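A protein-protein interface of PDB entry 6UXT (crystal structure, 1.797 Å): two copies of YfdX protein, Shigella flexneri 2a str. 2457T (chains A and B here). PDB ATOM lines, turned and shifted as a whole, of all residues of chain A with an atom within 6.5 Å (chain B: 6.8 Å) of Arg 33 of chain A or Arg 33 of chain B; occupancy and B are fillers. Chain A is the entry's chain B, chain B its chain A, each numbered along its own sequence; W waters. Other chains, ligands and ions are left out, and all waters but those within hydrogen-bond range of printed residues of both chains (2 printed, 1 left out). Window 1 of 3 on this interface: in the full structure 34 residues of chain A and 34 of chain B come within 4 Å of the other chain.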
ATOM      1  N   GLU A  26      33.249  26.173 -23.375  1.00  0.00           N
ATOM      2  CA  GLU A  26      32.128  27.106 -23.376  1.00  0.00           C
ATOM      3  C   GLU A  26      31.607  27.339 -24.785  1.00  0.00           C
ATOM      4  O   GLU A  26      30.409  27.622 -24.965  1.00  0.00           O
ATOM      5  CB  GLU A  26      32.533  28.423 -22.710  1.00  0.00           C
ATOM      6  CG  GLU A  26      33.022  28.245 -21.273  1.00  0.00           C
ATOM      7  CD  GLU A  26      31.914  27.867 -20.313  1.00  0.00           C
ATOM      8  OE1 GLU A  26      30.732  28.136 -20.623  1.00  0.00           O
ATOM      9  OE2 GLU A  26      32.228  27.299 -19.244  1.00  0.00           O
ATOM     10  N   GLY A  28      31.367  24.995 -27.245  1.00  0.00           N
ATOM     11  CA  GLY A  28      30.443  23.915 -27.551  1.00  0.00           C
ATOM     12  C   GLY A  28      29.140  24.029 -26.786  1.00  0.00           C
ATOM     13  O   GLY A  28      28.066  23.744 -27.327  1.00  0.00           O
ATOM     14  N   LEU A  29      29.214  24.427 -25.514  1.00  0.00           N
ATOM     15  CA  LEU A  29      27.995  24.578 -24.722  1.00  0.00           C
ATOM     16  C   LEU A  29      27.091  25.653 -25.305  1.00  0.00           C
ATOM     17  O   LEU A  29      25.871  25.467 -25.415  1.00  0.00           O
ATOM     18  CB  LEU A  29      28.343  24.922 -23.277  1.00  0.00           C
ATOM     19  CG  LEU A  29      27.159  25.087 -22.321  1.00  0.00           C
ATOM     20  CD1 LEU A  29      26.250  23.846 -22.312  1.00  0.00           C
ATOM     21  CD2 LEU A  29      27.669  25.407 -20.917  1.00  0.00           C
ATOM     22  N   TYR A  30      27.676  26.789 -25.682  1.00  0.00           N
ATOM     23  CA  TYR A  30      26.902  27.868 -26.287  1.00  0.00           C
ATOM     24  C   TYR A  30      26.224  27.408 -27.574  1.00  0.00           C
ATOM     25  O   TYR A  30      25.043  27.698 -27.812  1.00  0.00           O
ATOM     26  CB  TYR A  30      27.835  29.050 -26.554  1.00  0.00           C
ATOM     27  CG  TYR A  30      27.156  30.394 -26.650  1.00  0.00           C
ATOM     28  CD1 TYR A  30      27.091  31.236 -25.547  1.00  0.00           C
ATOM     29  CD2 TYR A  30      26.599  30.831 -27.844  1.00  0.00           C
ATOM     30  CE1 TYR A  30      26.476  32.481 -25.625  1.00  0.00           C
ATOM     31  CE2 TYR A  30      25.983  32.079 -27.933  1.00  0.00           C
ATOM     32  CZ  TYR A  30      25.925  32.896 -26.822  1.00  0.00           C
ATOM     33  OH  TYR A  30      25.322  34.133 -26.903  1.00  0.00           O
ATOM     34  N   ALA A  31      26.959  26.676 -28.412  1.00  0.00           N
ATOM     35  CA  ALA A  31      26.402  26.165 -29.658  1.00  0.00           C
ATOM     36  C   ALA A  31      25.191  25.274 -29.402  1.00  0.00           C
ATOM     37  O   ALA A  31      24.157  25.428 -30.050  1.00  0.00           O
ATOM     38  CB  ALA A  31      27.477  25.400 -30.432  1.00  0.00           C
ATOM     39  N   MET A  32      25.297  24.336 -28.454  1.00  0.00           N
ATOM     40  CA  MET A  32      24.157  23.448 -28.213  1.00  0.00           C
ATOM     41  C   MET A  32      22.987  24.205 -27.593  1.00  0.00           C
ATOM     42  O   MET A  32      21.829  23.861 -27.845  1.00  0.00           O
ATOM     43  CB  MET A  32      24.560  22.264 -27.327  1.00  0.00           C
ATOM     44  CG  MET A  32      25.612  21.341 -27.946  1.00  0.00           C
ATOM     45  SD  MET A  32      25.234  20.795 -29.616  1.00  0.00           S
ATOM     46  CE  MET A  32      23.698  19.922 -29.330  1.00  0.00           C
ATOM     47  N   ARG A  33      23.264  25.240 -26.783  1.00  0.00           N
ATOM     48  CA  ARG A  33      22.165  26.055 -26.269  1.00  0.00           C
ATOM     49  C   ARG A  33      21.471  26.821 -27.394  1.00  0.00           C
ATOM     50  O   ARG A  33      20.241  26.959 -27.384  1.00  0.00           O
ATOM     51  CB  ARG A  33      22.659  26.997 -25.168  1.00  0.00           C
ATOM     52  CG  ARG A  33      22.936  26.259 -23.862  1.00  0.00           C
ATOM     53  CD  ARG A  33      23.645  27.124 -22.813  1.00  0.00           C
ATOM     54  NE  ARG A  33      23.728  26.420 -21.531  1.00  0.00           N
ATOM     55  CZ  ARG A  33      24.410  26.864 -20.477  1.00  0.00           C
ATOM     56  NH1 ARG A  33      25.077  28.007 -20.544  1.00  0.00           N
ATOM     57  NH2 ARG A  33      24.420  26.167 -19.352  1.00  0.00           N
ATOM     58  N   ASP A  34      22.236  27.287 -28.387  1.00  0.00           N
ATOM     59  CA  ASP A  34      21.647  27.880 -29.589  1.00  0.00           C
ATOM     60  C   ASP A  34      20.747  26.889 -30.309  1.00  0.00           C
ATOM     61  O   ASP A  34      19.703  27.264 -30.851  1.00  0.00           O
ATOM     62  CB  ASP A  34      22.743  28.346 -30.551  1.00  0.00           C
ATOM     63  CG  ASP A  34      23.371  29.675 -30.152  1.00  0.00           C
ATOM     64  OD1 ASP A  34      22.845  30.358 -29.248  1.00  0.00           O
ATOM     65  OD2 ASP A  34      24.418  30.012 -30.744  1.00  0.00           O
ATOM     66  N   VAL A  35      21.163  25.622 -30.376  1.00  0.00           N
ATOM     67  CA  VAL A  35      20.359  24.625 -31.073  1.00  0.00           C
ATOM     68  C   VAL A  35      19.012  24.452 -30.385  1.00  0.00           C
ATOM     69  O   VAL A  35      17.975  24.317 -31.048  1.00  0.00           O
ATOM     70  CB  VAL A  35      21.130  23.293 -31.169  1.00  0.00           C
ATOM     71  CG1 VAL A  35      20.197  22.151 -31.567  1.00  0.00           C
ATOM     72  CG2 VAL A  35      22.269  23.433 -32.177  1.00  0.00           C
ATOM     73  N   GLN A  36      19.007  24.438 -29.045  1.00  0.00           N
ATOM     74  CA  GLN A  36      17.755  24.310 -28.296  1.00  0.00           C
ATOM     75  C   GLN A  36      16.799  25.455 -28.623  1.00  0.00           C
ATOM     76  O   GLN A  36      15.606  25.239 -28.880  1.00  0.00           O
ATOM     77  CB  GLN A  36      18.059  24.289 -26.797  1.00  0.00           C
ATOM     78  CG  GLN A  36      16.833  24.234 -25.884  1.00  0.00           C
ATOM     79  CD  GLN A  36      17.178  24.602 -24.452  1.00  0.00           C
ATOM     80  OE1 GLN A  36      18.348  24.573 -24.052  1.00  0.00           O
ATOM     81  NE2 GLN A  36      16.167  24.973 -23.676  1.00  0.00           N
ATOM     82  N   VAL A  37      17.306  26.687 -28.586  1.00  0.00           N
ATOM     83  CA  VAL A  37      16.461  27.846 -28.882  1.00  0.00           C
ATOM     84  C   VAL A  37      16.003  27.829 -30.339  1.00  0.00           C
ATOM     85  O   VAL A  37      14.871  28.227 -30.653  1.00  0.00           O
ATOM     86  CB  VAL A  37      17.194  29.156 -28.517  1.00  0.00           C
ATOM     87  CG1 VAL A  37      16.243  30.372 -28.714  1.00  0.00           C
ATOM     88  CG2 VAL A  37      17.657  29.102 -27.085  1.00  0.00           C
ATOM     89  N   ALA A  38      16.863  27.374 -31.254  1.00  0.00           N
ATOM     90  CA  ALA A  38      16.475  27.326 -32.658  1.00  0.00           C
ATOM     91  C   ALA A  38      15.290  26.396 -32.873  1.00  0.00           C
ATOM     92  O   ALA A  38      14.368  26.716 -33.635  1.00  0.00           O
ATOM     93  CB  ALA A  38      17.649  26.878 -33.523  1.00  0.00           C
ATOM     94  N   LEU A  53      20.202  31.450 -35.415  1.00  0.00           N
ATOM     95  CA  LEU A  53      20.759  30.671 -34.312  1.00  0.00           C
ATOM     96  C   LEU A  53      21.502  29.444 -34.813  1.00  0.00           C
ATOM     97  O   LEU A  53      22.534  29.059 -34.238  1.00  0.00           O
ATOM     98  CB  LEU A  53      19.642  30.261 -33.360  1.00  0.00           C
ATOM     99  CG  LEU A  53      19.201  31.321 -32.351  1.00  0.00           C
ATOM    100  CD1 LEU A  53      17.778  31.035 -31.886  1.00  0.00           C
ATOM    101  CD2 LEU A  53      20.186  31.394 -31.179  1.00  0.00           C
ATOM    102  N   ASN A  89      29.866  20.434 -20.639  1.00  0.00           N
ATOM    103  CA  ASN A  89      29.165  20.800 -19.416  1.00  0.00           C
ATOM    104  C   ASN A  89      29.547  19.788 -18.347  1.00  0.00           C
ATOM    105  O   ASN A  89      30.070  18.716 -18.652  1.00  0.00           O
ATOM    106  CB  ASN A  89      27.645  20.836 -19.616  1.00  0.00           C
ATOM    107  CG  ASN A  89      26.965  21.887 -18.756  1.00  0.00           C
ATOM    108  OD1 ASN A  89      27.574  22.467 -17.859  1.00  0.00           O
ATOM    109  ND2 ASN A  89      25.687  22.142 -19.039  1.00  0.00           N
ATOM    110  N   GLY B  28      15.735  33.784 -13.945  1.00  0.00           N
ATOM    111  CA  GLY B  28      15.665  32.472 -13.315  1.00  0.00           C
ATOM    112  C   GLY B  28      16.575  31.464 -13.988  1.00  0.00           C
ATOM    113  O   GLY B  28      17.235  30.661 -13.317  1.00  0.00           O
ATOM    114  N   LEU B  29      16.630  31.498 -15.322  1.00  0.00           N
ATOM    115  CA  LEU B  29      17.534  30.619 -16.056  1.00  0.00           C
ATOM    116  C   LEU B  29      18.980  30.828 -15.619  1.00  0.00           C
ATOM    117  O   LEU B  29      19.702  29.861 -15.329  1.00  0.00           O
ATOM    118  CB  LEU B  29      17.384  30.859 -17.555  1.00  0.00           C
ATOM    119  CG  LEU B  29      18.263  30.008 -18.469  1.00  0.00           C
ATOM    120  CD1 LEU B  29      17.955  28.513 -18.295  1.00  0.00           C
ATOM    121  CD2 LEU B  29      18.132  30.442 -19.917  1.00  0.00           C
ATOM    122  N   TYR B  30      19.423  32.090 -15.577  1.00  0.00           N
ATOM    123  CA  TYR B  30      20.804  32.385 -15.192  1.00  0.00           C
ATOM    124  C   TYR B  30      21.072  32.015 -13.740  1.00  0.00           C
ATOM    125  O   TYR B  30      22.179  31.581 -13.398  1.00  0.00           O
ATOM    126  CB  TYR B  30      21.120  33.866 -15.412  1.00  0.00           C
ATOM    127  CG  TYR B  30      21.177  34.310 -16.859  1.00  0.00           C
ATOM    128  CD1 TYR B  30      21.025  33.401 -17.901  1.00  0.00           C
ATOM    129  CD2 TYR B  30      21.388  35.645 -17.181  1.00  0.00           C
ATOM    130  CE1 TYR B  30      21.077  33.813 -19.225  1.00  0.00           C
ATOM    131  CE2 TYR B  30      21.441  36.067 -18.499  1.00  0.00           C
ATOM    132  CZ  TYR B  30      21.287  35.147 -19.515  1.00  0.00           C
ATOM    133  OH  TYR B  30      21.341  35.565 -20.826  1.00  0.00           O
ATOM    134  N   ALA B  31      20.086  32.216 -12.864  1.00  0.00           N
ATOM    135  CA  ALA B  31      20.275  31.877 -11.459  1.00  0.00           C
ATOM    136  C   ALA B  31      20.533  30.386 -11.287  1.00  0.00           C
ATOM    137  O   ALA B  31      21.461  29.987 -10.580  1.00  0.00           O
ATOM    138  CB  ALA B  31      19.057  32.307 -10.637  1.00  0.00           C
ATOM    139  N   MET B  32      19.726  29.541 -11.936  1.00  0.00           N
ATOM    140  CA  MET B  32      19.921  28.102 -11.765  1.00  0.00           C
ATOM    141  C   MET B  32      21.196  27.624 -12.458  1.00  0.00           C
ATOM    142  O   MET B  32      21.830  26.664 -12.000  1.00  0.00           O
ATOM    143  CB  MET B  32      18.681  27.344 -12.267  1.00  0.00           C
ATOM    144  CG  MET B  32      17.404  27.677 -11.479  1.00  0.00           C
ATOM    145  SD  MET B  32      17.599  27.623  -9.664  1.00  0.00           S
ATOM    146  CE  MET B  32      18.152  25.936  -9.389  1.00  0.00           C
ATOM    147  N   ARG B  33      21.599  28.276 -13.556  1.00  0.00           N
ATOM    148  CA  ARG B  33      22.902  27.962 -14.135  1.00  0.00           C
ATOM    149  C   ARG B  33      24.025  28.328 -13.173  1.00  0.00           C
ATOM    150  O   ARG B  33      24.988  27.567 -13.017  1.00  0.00           O
ATOM    151  CB  ARG B  33      23.078  28.666 -15.482  1.00  0.00           C
ATOM    152  CG  ARG B  33      22.199  28.059 -16.584  1.00  0.00           C
ATOM    153  CD  ARG B  33      22.347  28.827 -17.888  1.00  0.00           C
ATOM    154  NE  ARG B  33      21.633  28.182 -18.986  1.00  0.00           N
ATOM    155  CZ  ARG B  33      21.424  28.753 -20.170  1.00  0.00           C
ATOM    156  NH1 ARG B  33      21.879  29.977 -20.404  1.00  0.00           N
ATOM    157  NH2 ARG B  33      20.764  28.104 -21.118  1.00  0.00           N
ATOM    158  N   ASP B  34      23.894  29.468 -12.483  1.00  0.00           N
ATOM    159  CA  ASP B  34      24.883  29.841 -11.473  1.00  0.00           C
ATOM    160  C   ASP B  34      24.966  28.797 -10.370  1.00  0.00           C
ATOM    161  O   ASP B  34      26.059  28.486  -9.891  1.00  0.00           O
ATOM    162  CB  ASP B  34      24.555  31.203 -10.859  1.00  0.00           C
ATOM    163  CG  ASP B  34      24.781  32.359 -11.818  1.00  0.00           C
ATOM    164  OD1 ASP B  34      25.573  32.218 -12.771  1.00  0.00           O
ATOM    165  OD2 ASP B  34      24.152  33.415 -11.604  1.00  0.00           O
ATOM    166  N   VAL B  35      23.813  28.257  -9.950  1.00  0.00           N
ATOM    167  CA  VAL B  35      23.781  27.236  -8.904  1.00  0.00           C
ATOM    168  C   VAL B  35      24.557  26.001  -9.340  1.00  0.00           C
ATOM    169  O   VAL B  35      25.351  25.440  -8.573  1.00  0.00           O
ATOM    170  CB  VAL B  35      22.324  26.886  -8.543  1.00  0.00           C
ATOM    171  CG1 VAL B  35      22.267  25.641  -7.640  1.00  0.00           C
ATOM    172  CG2 VAL B  35      21.654  28.067  -7.859  1.00  0.00           C
ATOM    173  N   GLN B  36      24.318  25.540 -10.571  1.00  0.00           N
ATOM    174  CA  GLN B  36      25.037  24.366 -11.061  1.00  0.00           C
ATOM    175  C   GLN B  36      26.548  24.588 -11.019  1.00  0.00           C
ATOM    176  O   GLN B  36      27.303  23.734 -10.537  1.00  0.00           O
ATOM    177  CB  GLN B  36      24.583  24.046 -12.478  1.00  0.00           C
ATOM    178  CG  GLN B  36      25.415  22.971 -13.136  1.00  0.00           C
ATOM    179  CD  GLN B  36      25.334  23.020 -14.642  1.00  0.00           C
ATOM    180  OE1 GLN B  36      24.462  23.679 -15.206  1.00  0.00           O
ATOM    181  NE2 GLN B  36      26.259  22.342 -15.305  1.00  0.00           N
ATOM    182  N   VAL B  37      27.005  25.738 -11.512  1.00  0.00           N
ATOM    183  CA  VAL B  37      28.441  26.033 -11.525  1.00  0.00           C
ATOM    184  C   VAL B  37      28.980  26.195 -10.111  1.00  0.00           C
ATOM    185  O   VAL B  37      30.111  25.793  -9.815  1.00  0.00           O
ATOM    186  CB  VAL B  37      28.718  27.281 -12.390  1.00  0.00           C
ATOM    187  CG1 VAL B  37      30.227  27.591 -12.419  1.00  0.00           C
ATOM    188  CG2 VAL B  37      28.196  27.063 -13.819  1.00  0.00           C
ATOM    189  N   ALA B  38      28.193  26.787  -9.210  1.00  0.00           N
ATOM    190  CA  ALA B  38      28.657  26.954  -7.834  1.00  0.00           C
ATOM    191  C   ALA B  38      28.893  25.609  -7.143  1.00  0.00           C
ATOM    192  O   ALA B  38      29.850  25.458  -6.375  1.00  0.00           O
ATOM    193  CB  ALA B  38      27.653  27.784  -7.040  1.00  0.00           C
ATOM    194  N   LEU B  53      29.006  33.180  -7.173  1.00  0.00           N
ATOM    195  CA  LEU B  53      27.898  32.709  -8.003  1.00  0.00           C
ATOM    196  C   LEU B  53      26.608  32.582  -7.201  1.00  0.00           C
ATOM    197  O   LEU B  53      25.521  32.861  -7.723  1.00  0.00           O
ATOM    198  CB  LEU B  53      28.272  31.379  -8.649  1.00  0.00           C
ATOM    199  CG  LEU B  53      29.320  31.471  -9.755  1.00  0.00           C
ATOM    200  CD1 LEU B  53      29.949  30.119  -9.991  1.00  0.00           C
ATOM    201  CD2 LEU B  53      28.708  32.021 -11.035  1.00  0.00           C
ATOM    202  N   ASN B  89      12.860  27.870 -18.473  1.00  0.00           N
ATOM    203  CA  ASN B  89      13.476  27.275 -19.655  1.00  0.00           C
ATOM    204  C   ASN B  89      12.375  26.566 -20.430  1.00  0.00           C
ATOM    205  O   ASN B  89      11.298  26.306 -19.894  1.00  0.00           O
ATOM    206  CB  ASN B  89      14.599  26.295 -19.274  1.00  0.00           C
ATOM    207  CG  ASN B  89      15.698  26.237 -20.321  1.00  0.00           C
ATOM    208  OD1 ASN B  89      15.527  26.697 -21.448  1.00  0.00           O
ATOM    209  ND2 ASN B  89      16.845  25.683 -19.944  1.00  0.00           N
ATOM    210  N   GLU B 173      18.070  22.943  -6.676  1.00  0.00           N
ATOM    211  CA  GLU B 173      17.932  22.304  -7.978  1.00  0.00           C
ATOM    212  C   GLU B 173      16.775  21.316  -7.998  1.00  0.00           C
ATOM    213  O   GLU B 173      16.092  21.186  -9.017  1.00  0.00           O
ATOM    214  CB  GLU B 173      19.232  21.595  -8.355  1.00  0.00           C
ATOM    215  CG  GLU B 173      20.401  22.549  -8.532  1.00  0.00           C
ATOM    216  CD  GLU B 173      21.682  21.839  -8.943  1.00  0.00           C
ATOM    217  OE1 GLU B 173      21.928  20.717  -8.449  1.00  0.00           O
ATOM    218  OE2 GLU B 173      22.444  22.401  -9.764  1.00  0.00           O
HETATM  219  O   HOH W   1      16.784  28.403 -23.477  1.00  0.00           O
HETATM  220  O   HOH W   2      19.161  25.311 -21.707  1.00  0.00           O
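OD1 of Asn 89 of chain B is in hydrogen-bond range of NE2 of Gln 36 of chain A, at 2.9 Å.
The side-chain amide nitrogen of Gln 36 of chain B lies within hydrogen-bond range of the side-chain amide oxygen of Asn 89 of chain A.
NE of Arg 33 of chain A lies close to NH2 of Arg 33 of chain B (3.4 Å).
Of chain B, only Arg 33 (3.4 Å) comes within 4 Å of Arg 33 of chain A.
Of the printed residues of chain A, Arg 33 of chain B touches Arg 33 (3.4 Å).
Of the printed residues of chain B, Asn 89 of chain A touches Gln 36.
Of the printed residues of chain A, Asn 89 of chain B touches Gln 36.
Printed residues of chain B within 4 Å of Gln 36 of chain A: Asn 89 (2.9 Å).
Printed residues of chain A within 4 Å of Gln 36 of chain B: Asn 89.
Leu 53 of chain B touches none of the printed residues of chain A.
Asp 34 of chain A touches none of the printed residues of chain B.
The nearest residue of chain B that does not touch Arg 33 of chain A is Gln 36 of chain B (4.8 Å).
The nearest printed residue of chain B that does not touch Asn 89 of chain A is Val 37 of chain B (6.2 Å).
Among the printed residues, 3 pairs touch across the chains.
Among the printed residues, no Asp or Glu carboxylate lies within 4 Å of a Lys or Arg side-chain nitrogen of the other chain.
Arg 33 of chain A touches its own counterpart, Arg 33 of chain B.
Gln 36 of chain A touches Asn 89 of chain B, and with the chains exchanged Asn 89 of chain A touches Gln 36 of chain B.
13 positions are printed for both chains.
Water W2 lies within hydrogen-bond range of OE1 of Gln 36 of chain A (2.6 Å), ND2 of Asn 89 of chain B (2.9 Å) and NH2 of Arg 33 of chain B (3.3 Å).
Water W1 lies within hydrogen-bond range of the side-chain amide oxygen of Asn 89 of chain B and the side-chain amide nitrogen of Gln 36 of chain A.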
